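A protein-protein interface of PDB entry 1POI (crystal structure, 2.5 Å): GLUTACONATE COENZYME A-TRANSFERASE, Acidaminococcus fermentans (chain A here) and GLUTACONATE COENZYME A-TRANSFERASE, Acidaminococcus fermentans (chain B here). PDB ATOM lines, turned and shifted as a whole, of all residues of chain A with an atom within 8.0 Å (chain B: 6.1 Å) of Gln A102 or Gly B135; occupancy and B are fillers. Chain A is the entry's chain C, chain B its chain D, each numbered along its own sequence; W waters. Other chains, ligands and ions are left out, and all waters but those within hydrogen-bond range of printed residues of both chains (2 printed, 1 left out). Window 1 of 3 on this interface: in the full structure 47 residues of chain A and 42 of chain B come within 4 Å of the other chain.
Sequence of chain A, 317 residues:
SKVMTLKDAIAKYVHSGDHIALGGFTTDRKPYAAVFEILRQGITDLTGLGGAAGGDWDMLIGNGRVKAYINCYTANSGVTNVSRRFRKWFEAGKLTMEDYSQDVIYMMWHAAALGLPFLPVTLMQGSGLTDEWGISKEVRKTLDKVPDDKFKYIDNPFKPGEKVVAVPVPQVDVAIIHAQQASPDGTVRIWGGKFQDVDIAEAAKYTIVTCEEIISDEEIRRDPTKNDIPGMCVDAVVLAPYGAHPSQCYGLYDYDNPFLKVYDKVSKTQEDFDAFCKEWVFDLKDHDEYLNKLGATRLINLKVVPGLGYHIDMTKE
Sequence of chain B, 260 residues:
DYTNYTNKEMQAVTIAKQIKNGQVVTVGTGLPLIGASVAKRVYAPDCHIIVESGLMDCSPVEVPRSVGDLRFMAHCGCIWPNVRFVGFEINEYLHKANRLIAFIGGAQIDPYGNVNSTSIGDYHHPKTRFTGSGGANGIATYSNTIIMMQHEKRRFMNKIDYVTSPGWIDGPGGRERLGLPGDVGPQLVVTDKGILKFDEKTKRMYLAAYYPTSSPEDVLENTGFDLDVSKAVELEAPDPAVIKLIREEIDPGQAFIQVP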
ATOM      1  N   PHE A  25     -16.678  19.791 -14.561  1.00  0.00           N
ATOM      2  CA  PHE A  25     -16.516  19.411 -13.176  1.00  0.00           C
ATOM      3  C   PHE A  25     -15.929  18.006 -13.206  1.00  0.00           C
ATOM      4  O   PHE A  25     -16.611  17.070 -13.632  1.00  0.00           O
ATOM      5  CB  PHE A  25     -17.905  19.388 -12.544  1.00  0.00           C
ATOM      6  CG  PHE A  25     -17.920  19.280 -11.034  1.00  0.00           C
ATOM      7  CD1 PHE A  25     -17.966  18.029 -10.415  1.00  0.00           C
ATOM      8  CD2 PHE A  25     -18.015  20.430 -10.246  1.00  0.00           C
ATOM      9  CE1 PHE A  25     -18.117  17.926  -9.037  1.00  0.00           C
ATOM     10  CE2 PHE A  25     -18.168  20.331  -8.865  1.00  0.00           C
ATOM     11  CZ  PHE A  25     -18.222  19.076  -8.255  1.00  0.00           C
ATOM     12  N   THR A  26     -14.684  17.876 -12.740  1.00  0.00           N
ATOM     13  CA  THR A  26     -13.918  16.626 -12.736  1.00  0.00           C
ATOM     14  C   THR A  26     -14.097  15.779 -14.016  1.00  0.00           C
ATOM     15  O   THR A  26     -13.564  16.139 -15.059  1.00  0.00           O
ATOM     16  CB  THR A  26     -14.018  15.817 -11.378  1.00  0.00           C
ATOM     17  OG1 THR A  26     -15.289  15.160 -11.231  1.00  0.00           O
ATOM     18  CG2 THR A  26     -13.784  16.746 -10.198  1.00  0.00           C
ATOM     19  N   GLY A  51     -11.027  25.098  -9.987  1.00  0.00           N
ATOM     20  CA  GLY A  51     -12.426  24.700  -9.854  1.00  0.00           C
ATOM     21  C   GLY A  51     -12.320  23.239  -9.482  1.00  0.00           C
ATOM     22  O   GLY A  51     -11.246  22.819  -9.046  1.00  0.00           O
ATOM     23  N   ALA A  52     -13.388  22.467  -9.621  1.00  0.00           N
ATOM     24  CA  ALA A  52     -13.323  21.042  -9.306  1.00  0.00           C
ATOM     25  C   ALA A  52     -12.678  20.357 -10.524  1.00  0.00           C
ATOM     26  O   ALA A  52     -13.395  19.777 -11.359  1.00  0.00           O
ATOM     27  CB  ALA A  52     -14.709  20.499  -9.069  1.00  0.00           C
ATOM     28  N   ALA A  53     -11.336  20.424 -10.606  1.00  0.00           N
ATOM     29  CA  ALA A  53     -10.550  19.890 -11.736  1.00  0.00           C
ATOM     30  C   ALA A  53     -10.252  18.394 -11.829  1.00  0.00           C
ATOM     31  O   ALA A  53     -10.623  17.605 -10.961  1.00  0.00           O
ATOM     32  CB  ALA A  53      -9.272  20.656 -11.869  1.00  0.00           C
ATOM     33  N   ASN A  71      -6.003  26.106  -6.378  1.00  0.00           N
ATOM     34  CA  ASN A  71      -6.674  24.840  -6.140  1.00  0.00           C
ATOM     35  C   ASN A  71      -7.795  24.865  -5.120  1.00  0.00           C
ATOM     36  O   ASN A  71      -7.918  25.798  -4.324  1.00  0.00           O
ATOM     37  CB  ASN A  71      -5.655  23.790  -5.736  1.00  0.00           C
ATOM     38  CG  ASN A  71      -6.285  22.448  -5.476  1.00  0.00           C
ATOM     39  OD1 ASN A  71      -6.891  21.853  -6.370  1.00  0.00           O
ATOM     40  ND2 ASN A  71      -6.236  22.001  -4.227  1.00  0.00           N
ATOM     41  N   CYS A  72      -8.587  23.798  -5.141  1.00  0.00           N
ATOM     42  CA  CYS A  72      -9.715  23.601  -4.247  1.00  0.00           C
ATOM     43  C   CYS A  72     -10.014  22.109  -4.294  1.00  0.00           C
ATOM     44  O   CYS A  72     -10.584  21.550  -3.364  1.00  0.00           O
ATOM     45  CB  CYS A  72     -10.936  24.425  -4.724  1.00  0.00           C
ATOM     46  SG  CYS A  72     -12.177  23.524  -5.729  1.00  0.00           S
ATOM     47  N   TYR A  73      -9.593  21.468  -5.387  1.00  0.00           N
ATOM     48  CA  TYR A  73      -9.771  20.030  -5.629  1.00  0.00           C
ATOM     49  C   TYR A  73      -9.278  19.701  -7.029  1.00  0.00           C
ATOM     50  O   TYR A  73      -9.584  20.432  -7.977  1.00  0.00           O
ATOM     51  CB  TYR A  73     -11.238  19.654  -5.564  1.00  0.00           C
ATOM     52  CG  TYR A  73     -11.501  18.204  -5.812  1.00  0.00           C
ATOM     53  CD1 TYR A  73     -11.568  17.690  -7.098  1.00  0.00           C
ATOM     54  CD2 TYR A  73     -11.730  17.341  -4.752  1.00  0.00           C
ATOM     55  CE1 TYR A  73     -11.861  16.339  -7.325  1.00  0.00           C
ATOM     56  CE2 TYR A  73     -12.026  16.001  -4.961  1.00  0.00           C
ATOM     57  CZ  TYR A  73     -12.086  15.502  -6.251  1.00  0.00           C
ATOM     58  OH  TYR A  73     -12.328  14.160  -6.433  1.00  0.00           O
ATOM     59  N   THR A  74      -8.550  18.591  -7.162  1.00  0.00           N
ATOM     60  CA  THR A  74      -8.052  18.146  -8.462  1.00  0.00           C
ATOM     61  C   THR A  74      -7.989  16.626  -8.557  1.00  0.00           C
ATOM     62  O   THR A  74      -7.151  16.008  -7.908  1.00  0.00           O
ATOM     63  CB  THR A  74      -6.666  18.734  -8.762  1.00  0.00           C
ATOM     64  OG1 THR A  74      -6.736  20.162  -8.716  1.00  0.00           O
ATOM     65  CG2 THR A  74      -6.223  18.358 -10.155  1.00  0.00           C
ATOM     66  N   ASP A  99      -4.836  27.623  -1.935  1.00  0.00           N
ATOM     67  CA  ASP A  99      -5.948  26.766  -1.553  1.00  0.00           C
ATOM     68  C   ASP A  99      -7.082  27.592  -0.987  1.00  0.00           C
ATOM     69  O   ASP A  99      -6.854  28.434  -0.123  1.00  0.00           O
ATOM     70  CB  ASP A  99      -5.542  25.774  -0.456  1.00  0.00           C
ATOM     71  CG  ASP A  99      -4.748  24.586  -0.969  1.00  0.00           C
ATOM     72  OD1 ASP A  99      -5.356  23.709  -1.632  1.00  0.00           O
ATOM     73  OD2 ASP A  99      -3.533  24.501  -0.642  1.00  0.00           O
ATOM     74  N   TYR A 100      -8.273  27.402  -1.539  1.00  0.00           N
ATOM     75  CA  TYR A 100      -9.503  28.045  -1.053  1.00  0.00           C
ATOM     76  C   TYR A 100     -10.407  26.829  -1.007  1.00  0.00           C
ATOM     77  O   TYR A 100      -9.987  25.741  -1.403  1.00  0.00           O
ATOM     78  CB  TYR A 100     -10.082  29.026  -2.059  1.00  0.00           C
ATOM     79  CG  TYR A 100      -9.334  30.330  -2.202  1.00  0.00           C
ATOM     80  CD1 TYR A 100      -9.591  31.395  -1.358  1.00  0.00           C
ATOM     81  CD2 TYR A 100      -8.391  30.504  -3.200  1.00  0.00           C
ATOM     82  CE1 TYR A 100      -8.931  32.602  -1.499  1.00  0.00           C
ATOM     83  CE2 TYR A 100      -7.725  31.716  -3.355  1.00  0.00           C
ATOM     84  CZ  TYR A 100      -8.008  32.768  -2.498  1.00  0.00           C
ATOM     85  OH  TYR A 100      -7.408  34.003  -2.702  1.00  0.00           O
ATOM     86  N   SER A 101     -11.610  26.946  -0.481  1.00  0.00           N
ATOM     87  CA  SER A 101     -12.456  25.761  -0.500  1.00  0.00           C
ATOM     88  C   SER A 101     -13.103  25.733  -1.888  1.00  0.00           C
ATOM     89  O   SER A 101     -12.981  26.683  -2.660  1.00  0.00           O
ATOM     90  CB  SER A 101     -13.525  25.858   0.589  1.00  0.00           C
ATOM     91  OG  SER A 101     -14.143  27.133   0.562  1.00  0.00           O
ATOM     92  N   GLN A 102     -13.773  24.644  -2.221  1.00  0.00           N
ATOM     93  CA  GLN A 102     -14.459  24.579  -3.492  1.00  0.00           C
ATOM     94  C   GLN A 102     -15.610  25.587  -3.455  1.00  0.00           C
ATOM     95  O   GLN A 102     -15.860  26.282  -4.435  1.00  0.00           O
ATOM     96  CB  GLN A 102     -14.988  23.180  -3.732  1.00  0.00           C
ATOM     97  CG  GLN A 102     -15.505  22.941  -5.117  1.00  0.00           C
ATOM     98  CD  GLN A 102     -15.752  21.496  -5.332  1.00  0.00           C
ATOM     99  OE1 GLN A 102     -14.827  20.694  -5.413  1.00  0.00           O
ATOM    100  NE2 GLN A 102     -17.013  21.144  -5.467  1.00  0.00           N
ATOM    101  N   ASP A 103     -16.249  25.720  -2.294  1.00  0.00           N
ATOM    102  CA  ASP A 103     -17.348  26.656  -2.093  1.00  0.00           C
ATOM    103  C   ASP A 103     -16.916  28.051  -2.470  1.00  0.00           C
ATOM    104  O   ASP A 103     -17.614  28.758  -3.189  1.00  0.00           O
ATOM    105  CB  ASP A 103     -17.783  26.687  -0.623  1.00  0.00           C
ATOM    106  CG  ASP A 103     -17.996  25.312  -0.048  1.00  0.00           C
ATOM    107  OD1 ASP A 103     -18.982  24.657  -0.424  1.00  0.00           O
ATOM    108  OD2 ASP A 103     -17.165  24.865   0.767  1.00  0.00           O
ATOM    109  N   VAL A 104     -15.754  28.452  -1.983  1.00  0.00           N
ATOM    110  CA  VAL A 104     -15.249  29.793  -2.251  1.00  0.00           C
ATOM    111  C   VAL A 104     -14.718  29.979  -3.675  1.00  0.00           C
ATOM    112  O   VAL A 104     -14.543  31.112  -4.130  1.00  0.00           O
ATOM    113  CB  VAL A 104     -14.196  30.191  -1.186  1.00  0.00           C
ATOM    114  CG1 VAL A 104     -13.748  31.644  -1.334  1.00  0.00           C
ATOM    115  CG2 VAL A 104     -14.793  29.980   0.192  1.00  0.00           C
ATOM    116  N   ILE A 105     -14.482  28.880  -4.394  1.00  0.00           N
ATOM    117  CA  ILE A 105     -13.983  28.980  -5.769  1.00  0.00           C
ATOM    118  C   ILE A 105     -15.172  29.292  -6.631  1.00  0.00           C
ATOM    119  O   ILE A 105     -15.185  30.301  -7.351  1.00  0.00           O
ATOM    120  CB  ILE A 105     -13.350  27.684  -6.275  1.00  0.00           C
ATOM    121  CG1 ILE A 105     -12.004  27.451  -5.582  1.00  0.00           C
ATOM    122  CG2 ILE A 105     -13.175  27.750  -7.785  1.00  0.00           C
ATOM    123  CD1 ILE A 105     -11.027  28.613  -5.755  1.00  0.00           C
ATOM    124  N   TYR A 106     -16.187  28.439  -6.525  1.00  0.00           N
ATOM    125  CA  TYR A 106     -17.406  28.633  -7.288  1.00  0.00           C
ATOM    126  C   TYR A 106     -18.070  29.966  -6.969  1.00  0.00           C
ATOM    127  O   TYR A 106     -18.526  30.661  -7.877  1.00  0.00           O
ATOM    128  CB  TYR A 106     -18.347  27.455  -7.125  1.00  0.00           C
ATOM    129  CG  TYR A 106     -17.905  26.269  -7.958  1.00  0.00           C
ATOM    130  CD1 TYR A 106     -16.850  25.458  -7.557  1.00  0.00           C
ATOM    131  CD2 TYR A 106     -18.512  25.987  -9.180  1.00  0.00           C
ATOM    132  CE1 TYR A 106     -16.407  24.391  -8.362  1.00  0.00           C
ATOM    133  CE2 TYR A 106     -18.070  24.923  -9.991  1.00  0.00           C
ATOM    134  CZ  TYR A 106     -17.019  24.130  -9.577  1.00  0.00           C
ATOM    135  OH  TYR A 106     -16.580  23.087 -10.370  1.00  0.00           O
ATOM    136  N   MET A 107     -18.044  30.372  -5.702  1.00  0.00           N
ATOM    137  CA  MET A 107     -18.621  31.649  -5.314  1.00  0.00           C
ATOM    138  C   MET A 107     -17.791  32.776  -5.872  1.00  0.00           C
ATOM    139  O   MET A 107     -18.310  33.870  -6.066  1.00  0.00           O
ATOM    140  CB  MET A 107     -18.685  31.803  -3.794  1.00  0.00           C
ATOM    141  CG  MET A 107     -19.786  31.024  -3.084  1.00  0.00           C
ATOM    142  SD  MET A 107     -21.450  31.744  -3.207  1.00  0.00           S
ATOM    143  CE  MET A 107     -21.102  33.501  -3.714  1.00  0.00           C
ATOM    144  N   MET A 108     -16.501  32.533  -6.099  1.00  0.00           N
ATOM    145  CA  MET A 108     -15.589  33.561  -6.631  1.00  0.00           C
ATOM    146  C   MET A 108     -15.903  33.928  -8.080  1.00  0.00           C
ATOM    147  O   MET A 108     -16.007  35.107  -8.435  1.00  0.00           O
ATOM    148  CB  MET A 108     -14.132  33.100  -6.540  1.00  0.00           C
ATOM    149  CG  MET A 108     -13.431  33.489  -5.248  1.00  0.00           C
ATOM    150  SD  MET A 108     -11.806  32.707  -5.071  1.00  0.00           S
ATOM    151  CE  MET A 108     -10.745  33.919  -5.910  1.00  0.00           C
ATOM    152  N   TRP A 109     -16.040  32.904  -8.914  1.00  0.00           N
ATOM    153  CA  TRP A 109     -16.369  33.073 -10.321  1.00  0.00           C
ATOM    154  C   TRP A 109     -17.734  33.724 -10.490  1.00  0.00           C
ATOM    155  O   TRP A 109     -17.906  34.657 -11.288  1.00  0.00           O
ATOM    156  CB  TRP A 109     -16.399  31.715 -10.986  1.00  0.00           C
ATOM    157  CG  TRP A 109     -15.075  31.265 -11.475  1.00  0.00           C
ATOM    158  CD1 TRP A 109     -14.095  32.049 -12.021  1.00  0.00           C
ATOM    159  CD2 TRP A 109     -14.635  29.905 -11.615  1.00  0.00           C
ATOM    160  NE1 TRP A 109     -13.092  31.250 -12.523  1.00  0.00           N
ATOM    161  CE2 TRP A 109     -13.405  29.933 -12.287  1.00  0.00           C
ATOM    162  CE3 TRP A 109     -15.169  28.674 -11.244  1.00  0.00           C
ATOM    163  CZ2 TRP A 109     -12.703  28.771 -12.604  1.00  0.00           C
ATOM    164  CZ3 TRP A 109     -14.463  27.518 -11.561  1.00  0.00           C
ATOM    165  CH2 TRP A 109     -13.254  27.576 -12.235  1.00  0.00           C
ATOM    166  N   LEU A 123     -17.180  31.667   5.585  1.00  0.00           N
ATOM    167  CA  LEU A 123     -16.673  30.312   5.360  1.00  0.00           C
ATOM    168  C   LEU A 123     -15.142  30.426   5.364  1.00  0.00           C
ATOM    169  O   LEU A 123     -14.607  31.517   5.130  1.00  0.00           O
ATOM    170  CB  LEU A 123     -17.158  29.782   4.017  1.00  0.00           C
ATOM    171  CG  LEU A 123     -18.610  29.352   3.858  1.00  0.00           C
ATOM    172  CD1 LEU A 123     -18.981  29.468   2.395  1.00  0.00           C
ATOM    173  CD2 LEU A 123     -18.843  27.931   4.381  1.00  0.00           C
ATOM    174  N   MET A 124     -14.454  29.324   5.673  1.00  0.00           N
ATOM    175  CA  MET A 124     -12.975  29.260   5.726  1.00  0.00           C
ATOM    176  C   MET A 124     -12.274  29.725   7.021  1.00  0.00           C
ATOM    177  O   MET A 124     -11.048  29.602   7.139  1.00  0.00           O
ATOM    178  CB  MET A 124     -12.317  29.977   4.524  1.00  0.00           C
ATOM    179  CG  MET A 124     -12.658  29.407   3.139  1.00  0.00           C
ATOM    180  SD  MET A 124     -11.478  29.917   1.862  1.00  0.00           S
ATOM    181  CE  MET A 124     -11.264  31.678   2.130  1.00  0.00           C
ATOM    182  N   LEU A 129      -7.307  26.984   5.751  1.00  0.00           N
ATOM    183  CA  LEU A 129      -7.635  27.799   4.576  1.00  0.00           C
ATOM    184  C   LEU A 129      -7.357  29.285   4.811  1.00  0.00           C
ATOM    185  O   LEU A 129      -7.031  30.009   3.884  1.00  0.00           O
ATOM    186  CB  LEU A 129      -9.082  27.552   4.141  1.00  0.00           C
ATOM    187  CG  LEU A 129      -9.218  26.124   3.596  1.00  0.00           C
ATOM    188  CD1 LEU A 129     -10.616  25.618   3.642  1.00  0.00           C
ATOM    189  CD2 LEU A 129      -8.712  26.104   2.188  1.00  0.00           C
ATOM    190  N   GLU B  52     -22.463  17.966  -3.235  1.00  0.00           N
ATOM    191  CA  GLU B  52     -21.857  19.287  -3.394  1.00  0.00           C
ATOM    192  C   GLU B  52     -21.736  19.874  -4.793  1.00  0.00           C
ATOM    193  O   GLU B  52     -21.232  20.983  -4.964  1.00  0.00           O
ATOM    194  CB  GLU B  52     -20.504  19.320  -2.699  1.00  0.00           C
ATOM    195  CG  GLU B  52     -19.614  18.149  -3.064  1.00  0.00           C
ATOM    196  CD  GLU B  52     -18.272  18.215  -2.384  1.00  0.00           C
ATOM    197  OE1 GLU B  52     -17.633  19.291  -2.464  1.00  0.00           O
ATOM    198  OE2 GLU B  52     -17.862  17.195  -1.773  1.00  0.00           O
ATOM    199  N   SER B  53     -22.163  19.131  -5.801  1.00  0.00           N
ATOM    200  CA  SER B  53     -22.093  19.639  -7.165  1.00  0.00           C
ATOM    201  C   SER B  53     -23.324  20.493  -7.466  1.00  0.00           C
ATOM    202  O   SER B  53     -23.266  21.390  -8.315  1.00  0.00           O
ATOM    203  CB  SER B  53     -21.994  18.483  -8.141  1.00  0.00           C
ATOM    204  OG  SER B  53     -22.993  17.537  -7.843  1.00  0.00           O
ATOM    205  N   VAL B  67     -19.283  13.187  -8.005  1.00  0.00           N
ATOM    206  CA  VAL B  67     -20.437  13.945  -7.522  1.00  0.00           C
ATOM    207  C   VAL B  67     -21.184  14.648  -8.663  1.00  0.00           C
ATOM    208  O   VAL B  67     -22.324  15.073  -8.500  1.00  0.00           O
ATOM    209  CB  VAL B  67     -20.103  14.942  -6.371  1.00  0.00           C
ATOM    210  CG1 VAL B  67     -19.909  14.207  -5.109  1.00  0.00           C
ATOM    211  CG2 VAL B  67     -18.902  15.765  -6.682  1.00  0.00           C
ATOM    212  N   ASN B  82     -23.706  25.160  -8.523  1.00  0.00           N
ATOM    213  CA  ASN B  82     -22.880  24.834  -7.367  1.00  0.00           C
ATOM    214  C   ASN B  82     -23.175  25.775  -6.211  1.00  0.00           C
ATOM    215  O   ASN B  82     -23.611  25.334  -5.145  1.00  0.00           O
ATOM    216  CB  ASN B  82     -21.413  24.910  -7.765  1.00  0.00           C
ATOM    217  CG  ASN B  82     -21.119  24.086  -9.008  1.00  0.00           C
ATOM    218  OD1 ASN B  82     -20.362  23.117  -8.969  1.00  0.00           O
ATOM    219  ND2 ASN B  82     -21.715  24.478 -10.121  1.00  0.00           N
ATOM    220  N   PHE B  85     -25.914  25.321  -3.663  1.00  0.00           N
ATOM    221  CA  PHE B  85     -25.728  24.267  -2.662  1.00  0.00           C
ATOM    222  C   PHE B  85     -25.107  24.885  -1.396  1.00  0.00           C
ATOM    223  O   PHE B  85     -25.489  24.548  -0.267  1.00  0.00           O
ATOM    224  CB  PHE B  85     -24.836  23.147  -3.191  1.00  0.00           C
ATOM    225  CG  PHE B  85     -24.503  22.111  -2.168  1.00  0.00           C
ATOM    226  CD1 PHE B  85     -25.308  20.996  -2.003  1.00  0.00           C
ATOM    227  CD2 PHE B  85     -23.358  22.238  -1.379  1.00  0.00           C
ATOM    228  CE1 PHE B  85     -24.971  20.009  -1.055  1.00  0.00           C
ATOM    229  CE2 PHE B  85     -23.012  21.266  -0.435  1.00  0.00           C
ATOM    230  CZ  PHE B  85     -23.814  20.153  -0.271  1.00  0.00           C
ATOM    231  N   GLU B  89     -27.165  24.985   2.338  1.00  0.00           N
ATOM    232  CA  GLU B  89     -26.649  24.538   3.629  1.00  0.00           C
ATOM    233  C   GLU B  89     -26.551  25.705   4.627  1.00  0.00           C
ATOM    234  O   GLU B  89     -26.879  25.540   5.810  1.00  0.00           O
ATOM    235  CB  GLU B  89     -25.315  23.774   3.455  1.00  0.00           C
ATOM    236  CG  GLU B  89     -24.164  24.576   2.831  1.00  0.00           C
ATOM    237  CD  GLU B  89     -22.907  23.746   2.563  1.00  0.00           C
ATOM    238  OE1 GLU B  89     -22.971  22.494   2.615  1.00  0.00           O
ATOM    239  OE2 GLU B  89     -21.855  24.364   2.275  1.00  0.00           O
ATOM    240  N   SER B 133      -9.269  21.074   0.109  1.00  0.00           N
ATOM    241  CA  SER B 133     -10.545  21.229   0.785  1.00  0.00           C
ATOM    242  C   SER B 133     -11.763  20.554   0.165  1.00  0.00           C
ATOM    243  O   SER B 133     -12.433  19.752   0.820  1.00  0.00           O
ATOM    244  CB  SER B 133     -10.858  22.720   0.977  1.00  0.00           C
ATOM    245  OG  SER B 133     -12.250  22.964   1.177  1.00  0.00           O
ATOM    246  N   GLY B 134     -12.040  20.876  -1.099  1.00  0.00           N
ATOM    247  CA  GLY B 134     -13.240  20.376  -1.752  1.00  0.00           C
ATOM    248  C   GLY B 134     -14.316  21.255  -1.115  1.00  0.00           C
ATOM    249  O   GLY B 134     -14.067  22.428  -0.822  1.00  0.00           O
ATOM    250  N   GLY B 135     -15.496  20.705  -0.864  1.00  0.00           N
ATOM    251  CA  GLY B 135     -16.543  21.484  -0.216  1.00  0.00           C
ATOM    252  C   GLY B 135     -16.705  21.058   1.239  1.00  0.00           C
ATOM    253  O   GLY B 135     -17.625  21.492   1.936  1.00  0.00           O
ATOM    254  N   ALA B 136     -15.796  20.201   1.699  1.00  0.00           N
ATOM    255  CA  ALA B 136     -15.825  19.700   3.065  1.00  0.00           C
ATOM    256  C   ALA B 136     -15.573  20.835   4.016  1.00  0.00           C
ATOM    257  O   ALA B 136     -16.012  20.804   5.151  1.00  0.00           O
ATOM    258  CB  ALA B 136     -14.791  18.617   3.255  1.00  0.00           C
ATOM    259  N   ASN B 137     -14.857  21.849   3.574  1.00  0.00           N
ATOM    260  CA  ASN B 137     -14.651  22.954   4.478  1.00  0.00           C
ATOM    261  C   ASN B 137     -16.007  23.567   4.777  1.00  0.00           C
ATOM    262  O   ASN B 137     -16.357  23.753   5.941  1.00  0.00           O
ATOM    263  CB  ASN B 137     -13.748  24.026   3.899  1.00  0.00           C
ATOM    264  CG  ASN B 137     -13.717  25.250   4.764  1.00  0.00           C
ATOM    265  OD1 ASN B 137     -13.998  26.358   4.313  1.00  0.00           O
ATOM    266  ND2 ASN B 137     -13.407  25.055   6.032  1.00  0.00           N
ATOM    267  N   GLY B 138     -16.788  23.809   3.720  1.00  0.00           N
ATOM    268  CA  GLY B 138     -18.105  24.408   3.863  1.00  0.00           C
ATOM    269  C   GLY B 138     -19.052  23.556   4.675  1.00  0.00           C
ATOM    270  O   GLY B 138     -19.769  24.052   5.534  1.00  0.00           O
ATOM    271  N   ILE B 139     -19.053  22.264   4.399  1.00  0.00           N
ATOM    272  CA  ILE B 139     -19.895  21.333   5.120  1.00  0.00           C
ATOM    273  C   ILE B 139     -19.599  21.344   6.647  1.00  0.00           C
ATOM    274  O   ILE B 139     -20.520  21.261   7.471  1.00  0.00           O
ATOM    275  CB  ILE B 139     -19.675  19.933   4.560  1.00  0.00           C
ATOM    276  CG1 ILE B 139     -20.288  19.842   3.164  1.00  0.00           C
ATOM    277  CG2 ILE B 139     -20.220  18.886   5.502  1.00  0.00           C
ATOM    278  CD1 ILE B 139     -19.931  18.576   2.442  1.00  0.00           C
ATOM    279  N   ALA B 140     -18.315  21.454   6.996  1.00  0.00           N
ATOM    280  CA  ALA B 140     -17.848  21.459   8.371  1.00  0.00           C
ATOM    281  C   ALA B 140     -18.254  22.740   9.086  1.00  0.00           C
ATOM    282  O   ALA B 140     -18.574  22.732  10.280  1.00  0.00           O
ATOM    283  CB  ALA B 140     -16.334  21.308   8.389  1.00  0.00           C
HETATM  284  O   HOH W   1     -15.949  26.815   2.443  1.00  0.00           O
HETATM  285  O   HOH W   2     -19.490  23.247  -5.337  1.00  0.00           O
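O of Cys A72 is in hydrogen-bond range of N of Gly B134 (2.8 Å).
O of Gly B134 is in hydrogen-bond range of N of Gln A102.
OD2 of Asp A103 sits at hydrogen-bond distance from N of Gly B138 (3.2 Å).
The backbone NH (N) of Met A124 is in hydrogen-bond range of the side-chain amide oxygen (OD1) of Asn B137 (3.3 Å).
The side-chain hydroxyl of Tyr A106 is in hydrogen-bond range of the backbone NH of Ala A52, at 3.3 Å.
The backbone carbonyl oxygen (O) of Asn A71 lies within hydrogen-bond range of the backbone NH (N) of Tyr A100, 3.2 Å away.
SD of Met A124 is in hydrogen-bond range of N of Ser A101 (3.8 Å).
The backbone NH (N) of Gly B135 lies within hydrogen-bond range of the side-chain carboxylate (OE1) of Glu B52, 3.0 Å away.
The backbone carbonyl oxygen of Val B67 is in hydrogen-bond range of the side-chain hydroxyl of Ser B53.
O of Ser B53 lies close to OD1 of Asn B82, 3.4 Å away.
Among the printed residues, pairs that only touch across the chains: Phe A25 with Ser B53, Phe A25 with Val B67, Phe A25 with Asn B82, Cys A72 with Ser B133, Tyr A100 with Ser B133, Ser A101 with Ser B133, Ser A101 with Gly B134, Ser A101 with Asn B137, Gln A102 with Glu B52, Gln A102 with Gly B135, Asp A103 with Glu B89, Asp A103 with Gly B135, Tyr A106 with Asn B82, Leu A123 with Gly B138, Leu A129 with Ser B133 and Leu A129 with Asn B137.
Of the printed residues of chain B, Gln A102 touches Glu B52 (3.6 Å), Gly B134 (2.6 Å) and Gly B135 (3.8 Å).
Of the printed residues of chain A, Glu B52 touches Gln A102 (3.6 Å).
Of chain A, only Cys A72, Ser A101 and Gln A102 come within 4 Å of Gly B134.
Printed residues of chain A within 4 Å of Gly B135: Gln A102 and Asp A103.
No residue of chain A comes within 4 Å of Ala B136.
Of the printed residues of chain A, Asn B137 touches Ser A101 (3.8 Å), Met A124 (3.3 Å) and Leu A129 (3.3 Å).
Hydrophobic or aromatic side chains of chain B within 4 Å of the printed part of chain A: Val B67.
Among the printed residues, no Asp or Glu carboxylate lies within 4 Å of a Lys or Arg side-chain nitrogen of the other chain.
Water W1 lies within hydrogen-bond range of the side-chain hydroxyl (OG) of Ser A101 (2.6 Å), the side-chain amide oxygen (OD1) of Asn B137 (2.7 Å), the side-chain carboxylate (OD2) of Asp A103 (2.8 Å) and the backbone NH (N) of Gly B138 (3.4 Å).
Water W2 bridges the backbone carbonyl oxygen (O) of Glu B52 (2.9 Å) and the side-chain amide nitrogen (NE2) of Gln A102 (3.3 Å).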
